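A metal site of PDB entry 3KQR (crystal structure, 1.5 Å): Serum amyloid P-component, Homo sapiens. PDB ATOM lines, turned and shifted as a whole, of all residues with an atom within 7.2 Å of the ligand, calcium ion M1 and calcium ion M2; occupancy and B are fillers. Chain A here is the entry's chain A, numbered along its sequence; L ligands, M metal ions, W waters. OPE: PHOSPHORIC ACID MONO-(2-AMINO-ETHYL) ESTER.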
ATOM      1  N   ALA A  46     -27.364   3.511  -2.825  1.00  0.00           N
ATOM      2  CA  ALA A  46     -28.009   3.697  -4.111  1.00  0.00           C
ATOM      3  C   ALA A  46     -28.581   2.357  -4.580  1.00  0.00           C
ATOM      4  O   ALA A  46     -28.049   1.275  -4.241  1.00  0.00           O
ATOM      5  CB  ALA A  46     -27.002   4.214  -5.137  1.00  0.00           C
ATOM      6  N   TYR A  47     -29.639   2.420  -5.377  1.00  0.00           N
ATOM      7  CA  TYR A  47     -30.192   1.228  -5.963  1.00  0.00           C
ATOM      8  C   TYR A  47     -31.016   1.533  -7.205  1.00  0.00           C
ATOM      9  O   TYR A  47     -31.551   2.646  -7.373  1.00  0.00           O
ATOM     10  CB  TYR A  47     -31.050   0.439  -4.969  1.00  0.00           C
ATOM     11  CG  TYR A  47     -32.122   1.235  -4.249  1.00  0.00           C
ATOM     12  CD1 TYR A  47     -33.382   1.408  -4.805  1.00  0.00           C
ATOM     13  CD2 TYR A  47     -31.892   1.761  -2.975  1.00  0.00           C
ATOM     14  CE1 TYR A  47     -34.379   2.074  -4.098  1.00  0.00           C
ATOM     15  CE2 TYR A  47     -32.859   2.472  -2.275  1.00  0.00           C
ATOM     16  CZ  TYR A  47     -34.106   2.610  -2.830  1.00  0.00           C
ATOM     17  OH  TYR A  47     -35.065   3.263  -2.078  1.00  0.00           O
ATOM     18  N   SER A  48     -31.118   0.539  -8.087  1.00  0.00           N
ATOM     19  CA  SER A  48     -31.951   0.603  -9.253  1.00  0.00           C
ATOM     20  C   SER A  48     -33.412   0.252  -8.935  1.00  0.00           C
ATOM     21  O   SER A  48     -33.680  -0.745  -8.260  1.00  0.00           O
ATOM     22  CB  SER A  48     -31.437  -0.374 -10.303  1.00  0.00           C
ATOM     23  OG  SER A  48     -32.273  -0.374 -11.435  1.00  0.00           O
ATOM     24  N   SER A  51     -35.138  -1.113 -14.624  1.00  0.00           N
ATOM     25  CA  SER A  51     -34.027  -1.225 -15.559  1.00  0.00           C
ATOM     26  C   SER A  51     -34.532  -1.751 -16.899  1.00  0.00           C
ATOM     27  O   SER A  51     -35.089  -2.863 -16.981  1.00  0.00           O
ATOM     28  CB  SER A  51     -33.007  -2.170 -14.933  1.00  0.00           C
ATOM     29  OG  SER A  51     -31.918  -2.485 -15.783  1.00  0.00           O
ATOM     30  N   ASN A  53     -33.170  -2.297 -20.604  1.00  0.00           N
ATOM     31  CA  ASN A  53     -31.994  -2.339 -21.462  1.00  0.00           C
ATOM     32  C   ASN A  53     -32.435  -2.901 -22.805  1.00  0.00           C
ATOM     33  O   ASN A  53     -33.445  -3.590 -22.910  1.00  0.00           O
ATOM     34  CB  ASN A  53     -30.892  -3.181 -20.805  1.00  0.00           C
ATOM     35  CG  ASN A  53     -29.935  -2.352 -19.979  1.00  0.00           C
ATOM     36  OD1 ASN A  53     -30.216  -1.189 -19.640  1.00  0.00           O
ATOM     37  ND2 ASN A  53     -28.780  -2.937 -19.651  1.00  0.00           N
ATOM     38  N   ASP A  58     -26.973  -0.189 -22.823  1.00  0.00           N
ATOM     39  CA  ASP A  58     -27.119  -0.145 -21.358  1.00  0.00           C
ATOM     40  C   ASP A  58     -27.865   1.141 -20.977  1.00  0.00           C
ATOM     41  O   ASP A  58     -27.742   2.178 -21.656  1.00  0.00           O
ATOM     42  CB  ASP A  58     -25.740  -0.138 -20.663  1.00  0.00           C
ATOM     43  CG  ASP A  58     -25.818  -0.358 -19.141  1.00  0.00           C
ATOM     44  OD1 ASP A  58     -26.732  -1.074 -18.711  1.00  0.00           O
ATOM     45  OD2 ASP A  58     -24.965   0.163 -18.378  1.00  0.00           O
ATOM     46  N   ASN A  59     -28.573   1.078 -19.849  1.00  0.00           N
ATOM     47  CA  ASN A  59     -29.265   2.230 -19.274  1.00  0.00           C
ATOM     48  C   ASN A  59     -30.157   2.901 -20.301  1.00  0.00           C
ATOM     49  O   ASN A  59     -30.127   4.132 -20.425  1.00  0.00           O
ATOM     50  CB  ASN A  59     -28.248   3.202 -18.642  1.00  0.00           C
ATOM     51  CG  ASN A  59     -27.427   2.535 -17.526  1.00  0.00           C
ATOM     52  OD1 ASN A  59     -27.722   1.406 -17.132  1.00  0.00           O
ATOM     53  ND2 ASN A  59     -26.437   3.227 -17.016  1.00  0.00           N
ATOM     54  N   GLU A  60     -30.892   2.106 -21.091  1.00  0.00           N
ATOM     55  CA  GLU A  60     -31.684   2.716 -22.168  1.00  0.00           C
ATOM     56  C   GLU A  60     -32.807   3.509 -21.540  1.00  0.00           C
ATOM     57  O   GLU A  60     -33.096   4.629 -21.962  1.00  0.00           O
ATOM     58  CB  GLU A  60     -32.183   1.725 -23.235  1.00  0.00           C
ATOM     59  CG  GLU A  60     -33.017   2.329 -24.349  1.00  0.00           C
ATOM     60  CD  GLU A  60     -32.218   3.179 -25.329  1.00  0.00           C
ATOM     61  OE1 GLU A  60     -30.972   3.278 -25.158  1.00  0.00           O
ATOM     62  OE2 GLU A  60     -32.858   3.684 -26.252  1.00  0.00           O
ATOM     63  N   LEU A  62     -33.658   3.960 -17.369  1.00  0.00           N
ATOM     64  CA  LEU A  62     -33.338   3.490 -16.032  1.00  0.00           C
ATOM     65  C   LEU A  62     -33.837   4.490 -15.001  1.00  0.00           C
ATOM     66  O   LEU A  62     -33.547   5.696 -15.104  1.00  0.00           O
ATOM     67  CB  LEU A  62     -31.811   3.318 -15.879  1.00  0.00           C
ATOM     68  CG  LEU A  62     -31.258   3.038 -14.488  1.00  0.00           C
ATOM     69  CD1 LEU A  62     -31.727   1.712 -13.904  1.00  0.00           C
ATOM     70  CD2 LEU A  62     -29.733   3.056 -14.468  1.00  0.00           C
ATOM     71  N   TYR A  64     -33.406   5.313 -11.101  1.00  0.00           N
ATOM     72  CA  TYR A  64     -32.350   4.994 -10.148  1.00  0.00           C
ATOM     73  C   TYR A  64     -32.434   5.925  -8.953  1.00  0.00           C
ATOM     74  O   TYR A  64     -32.649   7.109  -9.106  1.00  0.00           O
ATOM     75  CB  TYR A  64     -30.980   5.191 -10.840  1.00  0.00           C
ATOM     76  CG  TYR A  64     -29.792   4.573 -10.119  1.00  0.00           C
ATOM     77  CD1 TYR A  64     -29.575   3.198 -10.186  1.00  0.00           C
ATOM     78  CD2 TYR A  64     -28.888   5.344  -9.418  1.00  0.00           C
ATOM     79  CE1 TYR A  64     -28.501   2.620  -9.567  1.00  0.00           C
ATOM     80  CE2 TYR A  64     -27.774   4.757  -8.799  1.00  0.00           C
ATOM     81  CZ  TYR A  64     -27.616   3.397  -8.888  1.00  0.00           C
ATOM     82  OH  TYR A  64     -26.533   2.762  -8.271  1.00  0.00           O
ATOM     83  N   GLU A  66     -30.365   7.551  -6.162  1.00  0.00           N
ATOM     84  CA  GLU A  66     -28.981   7.879  -5.826  1.00  0.00           C
ATOM     85  C   GLU A  66     -28.716   7.836  -4.308  1.00  0.00           C
ATOM     86  O   GLU A  66     -27.717   7.286  -3.800  1.00  0.00           O
ATOM     87  CB  GLU A  66     -28.723   9.320  -6.308  1.00  0.00           C
ATOM     88  CG  GLU A  66     -29.060   9.611  -7.783  1.00  0.00           C
ATOM     89  CD  GLU A  66     -28.063   8.947  -8.746  1.00  0.00           C
ATOM     90  OE1 GLU A  66     -27.070   8.366  -8.238  1.00  0.00           O
ATOM     91  OE2 GLU A  66     -28.272   9.011 -10.000  1.00  0.00           O
ATOM     92  N   SER A  72     -33.268   9.740 -10.120  1.00  0.00           N
ATOM     93  CA  SER A  72     -32.698   9.922 -11.441  1.00  0.00           C
ATOM     94  C   SER A  72     -33.395   9.114 -12.506  1.00  0.00           C
ATOM     95  O   SER A  72     -33.832   7.987 -12.273  1.00  0.00           O
ATOM     96  CB  SER A  72     -31.228   9.527 -11.450  1.00  0.00           C
ATOM     97  OG  SER A  72     -30.488  10.345 -10.540  1.00  0.00           O
ATOM     98  N   TYR A  74     -32.451   7.880 -16.424  1.00  0.00           N
ATOM     99  CA  TYR A  74     -31.570   7.790 -17.574  1.00  0.00           C
ATOM    100  C   TYR A  74     -32.369   7.473 -18.807  1.00  0.00           C
ATOM    101  O   TYR A  74     -33.262   6.611 -18.785  1.00  0.00           O
ATOM    102  CB  TYR A  74     -30.555   6.671 -17.385  1.00  0.00           C
ATOM    103  CG  TYR A  74     -29.545   6.869 -16.295  1.00  0.00           C
ATOM    104  CD1 TYR A  74     -29.888   6.801 -14.978  1.00  0.00           C
ATOM    105  CD2 TYR A  74     -28.206   7.071 -16.614  1.00  0.00           C
ATOM    106  CE1 TYR A  74     -28.937   6.957 -13.975  1.00  0.00           C
ATOM    107  CE2 TYR A  74     -27.258   7.221 -15.629  1.00  0.00           C
ATOM    108  CZ  TYR A  74     -27.618   7.166 -14.316  1.00  0.00           C
ATOM    109  OH  TYR A  74     -26.661   7.304 -13.328  1.00  0.00           O
ATOM    110  N   ARG A  77     -28.510   6.513 -21.769  1.00  0.00           N
ATOM    111  CA  ARG A  77     -27.248   6.796 -21.100  1.00  0.00           C
ATOM    112  C   ARG A  77     -27.065   8.224 -20.581  1.00  0.00           C
ATOM    113  O   ARG A  77     -26.166   8.481 -19.802  1.00  0.00           O
ATOM    114  CB  ARG A  77     -26.065   6.434 -22.025  1.00  0.00           C
ATOM    115  CG  ARG A  77     -25.924   4.943 -22.183  1.00  0.00           C
ATOM    116  CD  ARG A  77     -25.187   4.412 -20.982  1.00  0.00           C
ATOM    117  NE  ARG A  77     -23.795   4.825 -20.997  1.00  0.00           N
ATOM    118  CZ  ARG A  77     -22.795   4.030 -21.349  1.00  0.00           C
ATOM    119  NH1 ARG A  77     -23.044   2.772 -21.711  1.00  0.00           N
ATOM    120  NH2 ARG A  77     -21.555   4.494 -21.340  1.00  0.00           N
ATOM    121  N   LYS A  79     -28.593  11.367 -18.253  1.00  0.00           N
ATOM    122  CA  LYS A  79     -29.392  11.362 -17.022  1.00  0.00           C
ATOM    123  C   LYS A  79     -29.804  12.733 -16.578  1.00  0.00           C
ATOM    124  O   LYS A  79     -29.179  13.780 -16.892  1.00  0.00           O
ATOM    125  CB  LYS A  79     -28.696  10.635 -15.875  1.00  0.00           C
ATOM    126  CG  LYS A  79     -27.499  11.344 -15.407  1.00  0.00           C
ATOM    127  CD  LYS A  79     -26.762  10.565 -14.319  1.00  0.00           C
ATOM    128  CE  LYS A  79     -27.535  10.588 -13.025  1.00  0.00           C
ATOM    129  NZ  LYS A  79     -26.640  10.181 -11.901  1.00  0.00           N
ATOM    130  N   GLU A 136     -29.974  -4.027 -11.411  1.00  0.00           N
ATOM    131  CA  GLU A 136     -29.594  -3.129 -12.464  1.00  0.00           C
ATOM    132  C   GLU A 136     -28.835  -3.909 -13.549  1.00  0.00           C
ATOM    133  O   GLU A 136     -27.862  -4.586 -13.250  1.00  0.00           O
ATOM    134  CB  GLU A 136     -28.705  -2.037 -11.844  1.00  0.00           C
ATOM    135  CG  GLU A 136     -28.774  -0.746 -12.558  1.00  0.00           C
ATOM    136  CD  GLU A 136     -27.926  -0.750 -13.789  1.00  0.00           C
ATOM    137  OE1 GLU A 136     -26.757  -1.219 -13.696  1.00  0.00           O
ATOM    138  OE2 GLU A 136     -28.387  -0.266 -14.844  1.00  0.00           O
ATOM    139  N   GLN A 137     -29.309  -3.838 -14.786  1.00  0.00           N
ATOM    140  CA  GLN A 137     -28.672  -4.569 -15.869  1.00  0.00           C
ATOM    141  C   GLN A 137     -27.474  -3.814 -16.355  1.00  0.00           C
ATOM    142  O   GLN A 137     -27.539  -2.597 -16.509  1.00  0.00           O
ATOM    143  CB  GLN A 137     -29.617  -4.748 -17.046  1.00  0.00           C
ATOM    144  CG  GLN A 137     -30.850  -5.574 -16.766  1.00  0.00           C
ATOM    145  CD  GLN A 137     -31.798  -5.522 -17.940  1.00  0.00           C
ATOM    146  OE1 GLN A 137     -31.653  -6.262 -18.910  1.00  0.00           O
ATOM    147  NE2 GLN A 137     -32.760  -4.595 -17.883  1.00  0.00           N
ATOM    148  N   ASP A 138     -26.403  -4.512 -16.641  1.00  0.00           N
ATOM    149  CA  ASP A 138     -25.309  -3.914 -17.403  1.00  0.00           C
ATOM    150  C   ASP A 138     -25.194  -4.602 -18.773  1.00  0.00           C
ATOM    151  O   ASP A 138     -24.427  -4.159 -19.637  1.00  0.00           O
ATOM    152  CB  ASP A 138     -23.992  -3.963 -16.630  1.00  0.00           C
ATOM    153  CG  ASP A 138     -23.891  -2.874 -15.579  1.00  0.00           C
ATOM    154  OD1 ASP A 138     -24.702  -1.908 -15.654  1.00  0.00           O
ATOM    155  OD2 ASP A 138     -23.016  -2.935 -14.674  1.00  0.00           O
ATOM    156  N   SER A 139     -25.994  -5.657 -18.986  1.00  0.00           N
ATOM    157  CA  SER A 139     -26.087  -6.313 -20.299  1.00  0.00           C
ATOM    158  C   SER A 139     -27.553  -6.443 -20.731  1.00  0.00           C
ATOM    159  O   SER A 139     -28.446  -5.967 -20.038  1.00  0.00           O
ATOM    160  CB  SER A 139     -25.452  -7.689 -20.224  1.00  0.00           C
ATOM    161  OG  SER A 139     -26.310  -8.573 -19.515  1.00  0.00           O
ATOM    162  N   GLY A 142     -28.828  -9.092 -18.049  1.00  0.00           N
ATOM    163  CA  GLY A 142     -27.950  -9.578 -17.001  1.00  0.00           C
ATOM    164  C   GLY A 142     -26.854  -8.623 -16.572  1.00  0.00           C
ATOM    165  O   GLY A 142     -27.032  -7.407 -16.590  1.00  0.00           O
ATOM    166  N   LYS A 143     -25.715  -9.185 -16.166  1.00  0.00           N
ATOM    167  CA  LYS A 143     -24.595  -8.407 -15.643  1.00  0.00           C
ATOM    168  C   LYS A 143     -25.028  -7.533 -14.476  1.00  0.00           C
ATOM    169  O   LYS A 143     -24.828  -6.315 -14.480  1.00  0.00           O
ATOM    170  CB  LYS A 143     -23.971  -7.518 -16.731  1.00  0.00           C
ATOM    171  CG  LYS A 143     -23.048  -8.248 -17.708  1.00  0.00           C
ATOM    172  CD  LYS A 143     -21.595  -8.128 -17.282  1.00  0.00           C
ATOM    173  CE  LYS A 143     -20.650  -8.557 -18.400  1.00  0.00           C
ATOM    174  NZ  LYS A 143     -20.666  -7.602 -19.551  1.00  0.00           N
ATOM    175  N   PHE A 144     -25.640  -8.166 -13.481  1.00  0.00           N
ATOM    176  CA  PHE A 144     -26.082  -7.483 -12.277  1.00  0.00           C
ATOM    177  C   PHE A 144     -24.936  -7.117 -11.331  1.00  0.00           C
ATOM    178  O   PHE A 144     -23.816  -7.582 -11.460  1.00  0.00           O
ATOM    179  CB  PHE A 144     -27.120  -8.353 -11.571  1.00  0.00           C
ATOM    180  CG  PHE A 144     -28.256  -8.813 -12.473  1.00  0.00           C
ATOM    181  CD1 PHE A 144     -28.794  -7.961 -13.431  1.00  0.00           C
ATOM    182  CD2 PHE A 144     -28.793 -10.078 -12.342  1.00  0.00           C
ATOM    183  CE1 PHE A 144     -29.858  -8.370 -14.240  1.00  0.00           C
ATOM    184  CE2 PHE A 144     -29.841 -10.508 -13.144  1.00  0.00           C
ATOM    185  CZ  PHE A 144     -30.379  -9.657 -14.102  1.00  0.00           C
ATOM    186  N   ASP A 145     -25.239  -6.260 -10.370  1.00  0.00           N
ATOM    187  CA  ASP A 145     -24.278  -5.752  -9.409  1.00  0.00           C
ATOM    188  C   ASP A 145     -24.971  -5.692  -8.060  1.00  0.00           C
ATOM    189  O   ASP A 145     -25.942  -4.950  -7.893  1.00  0.00           O
ATOM    190  CB  ASP A 145     -23.826  -4.357  -9.846  1.00  0.00           C
ATOM    191  CG  ASP A 145     -22.898  -3.666  -8.852  1.00  0.00           C
ATOM    192  OD1 ASP A 145     -22.768  -4.121  -7.697  1.00  0.00           O
ATOM    193  OD2 ASP A 145     -22.286  -2.635  -9.245  1.00  0.00           O
ATOM    194  N   GLN A 148     -26.104  -2.466  -6.397  1.00  0.00           N
ATOM    195  CA  GLN A 148     -27.219  -1.691  -6.976  1.00  0.00           C
ATOM    196  C   GLN A 148     -28.547  -2.434  -6.879  1.00  0.00           C
ATOM    197  O   GLN A 148     -29.574  -1.969  -7.397  1.00  0.00           O
ATOM    198  CB  GLN A 148     -26.971  -1.388  -8.445  1.00  0.00           C
ATOM    199  CG  GLN A 148     -25.649  -0.721  -8.663  1.00  0.00           C
ATOM    200  CD  GLN A 148     -25.411  -0.467 -10.092  1.00  0.00           C
ATOM    201  OE1 GLN A 148     -25.347  -1.398 -10.891  1.00  0.00           O
ATOM    202  NE2 GLN A 148     -25.318   0.821 -10.464  1.00  0.00           N
HETATM  203  CA  OPE L   1     -26.240   3.260 -13.443  1.00  0.00           C
HETATM  204  CB  OPE L   1     -26.647   4.118 -12.273  1.00  0.00           C
HETATM  205  O1  OPE L   1     -23.668   0.392 -13.231  1.00  0.00           O
HETATM  206  O2  OPE L   1     -23.164   2.525 -14.490  1.00  0.00           O
HETATM  207  O3  OPE L   1     -25.136   1.132 -15.210  1.00  0.00           O
HETATM  208  O4  OPE L   1     -25.216   2.439 -12.947  1.00  0.00           O
HETATM  209  N   OPE L   1     -25.472   4.911 -11.855  1.00  0.00           N
HETATM  210  P   OPE L   1     -24.375   1.559 -14.023  1.00  0.00           P
HETATM  211 CA    CA M   1     -26.478  -0.473 -16.262  1.00  0.00          CA
HETATM  212 CA    CA M   2     -24.548  -1.741 -13.084  1.00  0.00          CA
HETATM  213  O   HOH W   1     -25.286  -4.075 -12.843  1.00  0.00           O
HETATM  214  O   HOH W   2     -23.677   3.723 -10.314  1.00  0.00           O
HETATM  215  O   HOH W   3     -22.509  -2.046 -11.867  1.00  0.00           O
HETATM  216  O   HOH W   4     -22.148   1.385 -11.185  1.00  0.00           O
HETATM  217  O   HOH W   5     -25.459   7.111 -10.035  1.00  0.00           O
HETATM  218  O   HOH W   6     -22.751   1.842 -17.225  1.00  0.00           O
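N of the ligand is in hydrogen-bond range of OH of Tyr 74 (3.1 Å).
NE2 of Gln 148 lies within hydrogen-bond range of OH of Tyr 64 (3.2 Å). The backbone NH (N) of Ser 48 is in hydrogen-bond range of the backbone carbonyl oxygen (O) of Gln 148. The backbone NH of Asp 138 lies within hydrogen-bond range of the backbone carbonyl oxygen of Lys 143 (3.2 Å). The side-chain amide nitrogen of Asn 53 lies close to the backbone carbonyl oxygen of Gln 137, at 3.4 Å. The side-chain amide nitrogen (NE2) of Gln 137 is in hydrogen-bond range of the backbone carbonyl oxygen (O) of Ser 51 (3.0 Å). O of Ser 139 lies close to OE1 of Gln 137 (3.4 Å). O of Asn 59 lies within hydrogen-bond range of N of Arg 77 (3.2 Å). N of Tyr 74 is in hydrogen-bond range of O of Leu 62 (2.8 Å).
Leu 62 touches the ligand (CD2 to CA, 3.6 Å). Tyr 64 touches the ligand (CZ to CB, 3.6 Å). Hydrophobic or aromatic side chains that line the ligand: Leu 62, Tyr 64 and Tyr 74.
Three residues have an atom within 4 Å of calcium ion M2: Glu 136, Asp 138 and Gln 148. The nearest printed residue that does not touch calcium ion M2 is Asp 145 (4.2 Å).
Calcium ion M1 is bound by O3 of the ligand, OD1 of Asp 138, OE2 of Glu 136, O of Gln 137, OD1 of Asn 59, OD1 of Asp 58, OD2 of Asp 58 and OE1 of Glu 136. Calcium ion M1 has eight donor atoms within binding distance.
Calcium ion M2 is bound by O1 of the ligand, OE1 of Glu 136, OE1 of Gln 148, water W3, water W1, OD2 of Asp 138 and OD1 of Asp 138.
Water W1 lies within hydrogen-bond range of O of Glu 136, O of Lys 143 and N of Asp 145. Water W2 bridges a nitrogen (N) of the ligand (2.6 Å) and the side-chain amide nitrogen (NE2) of Gln 148 (3.3 Å). Water W5 lies within hydrogen-bond range of OE1 of Glu 66 (2.7 Å) and N of the ligand (2.9 Å).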
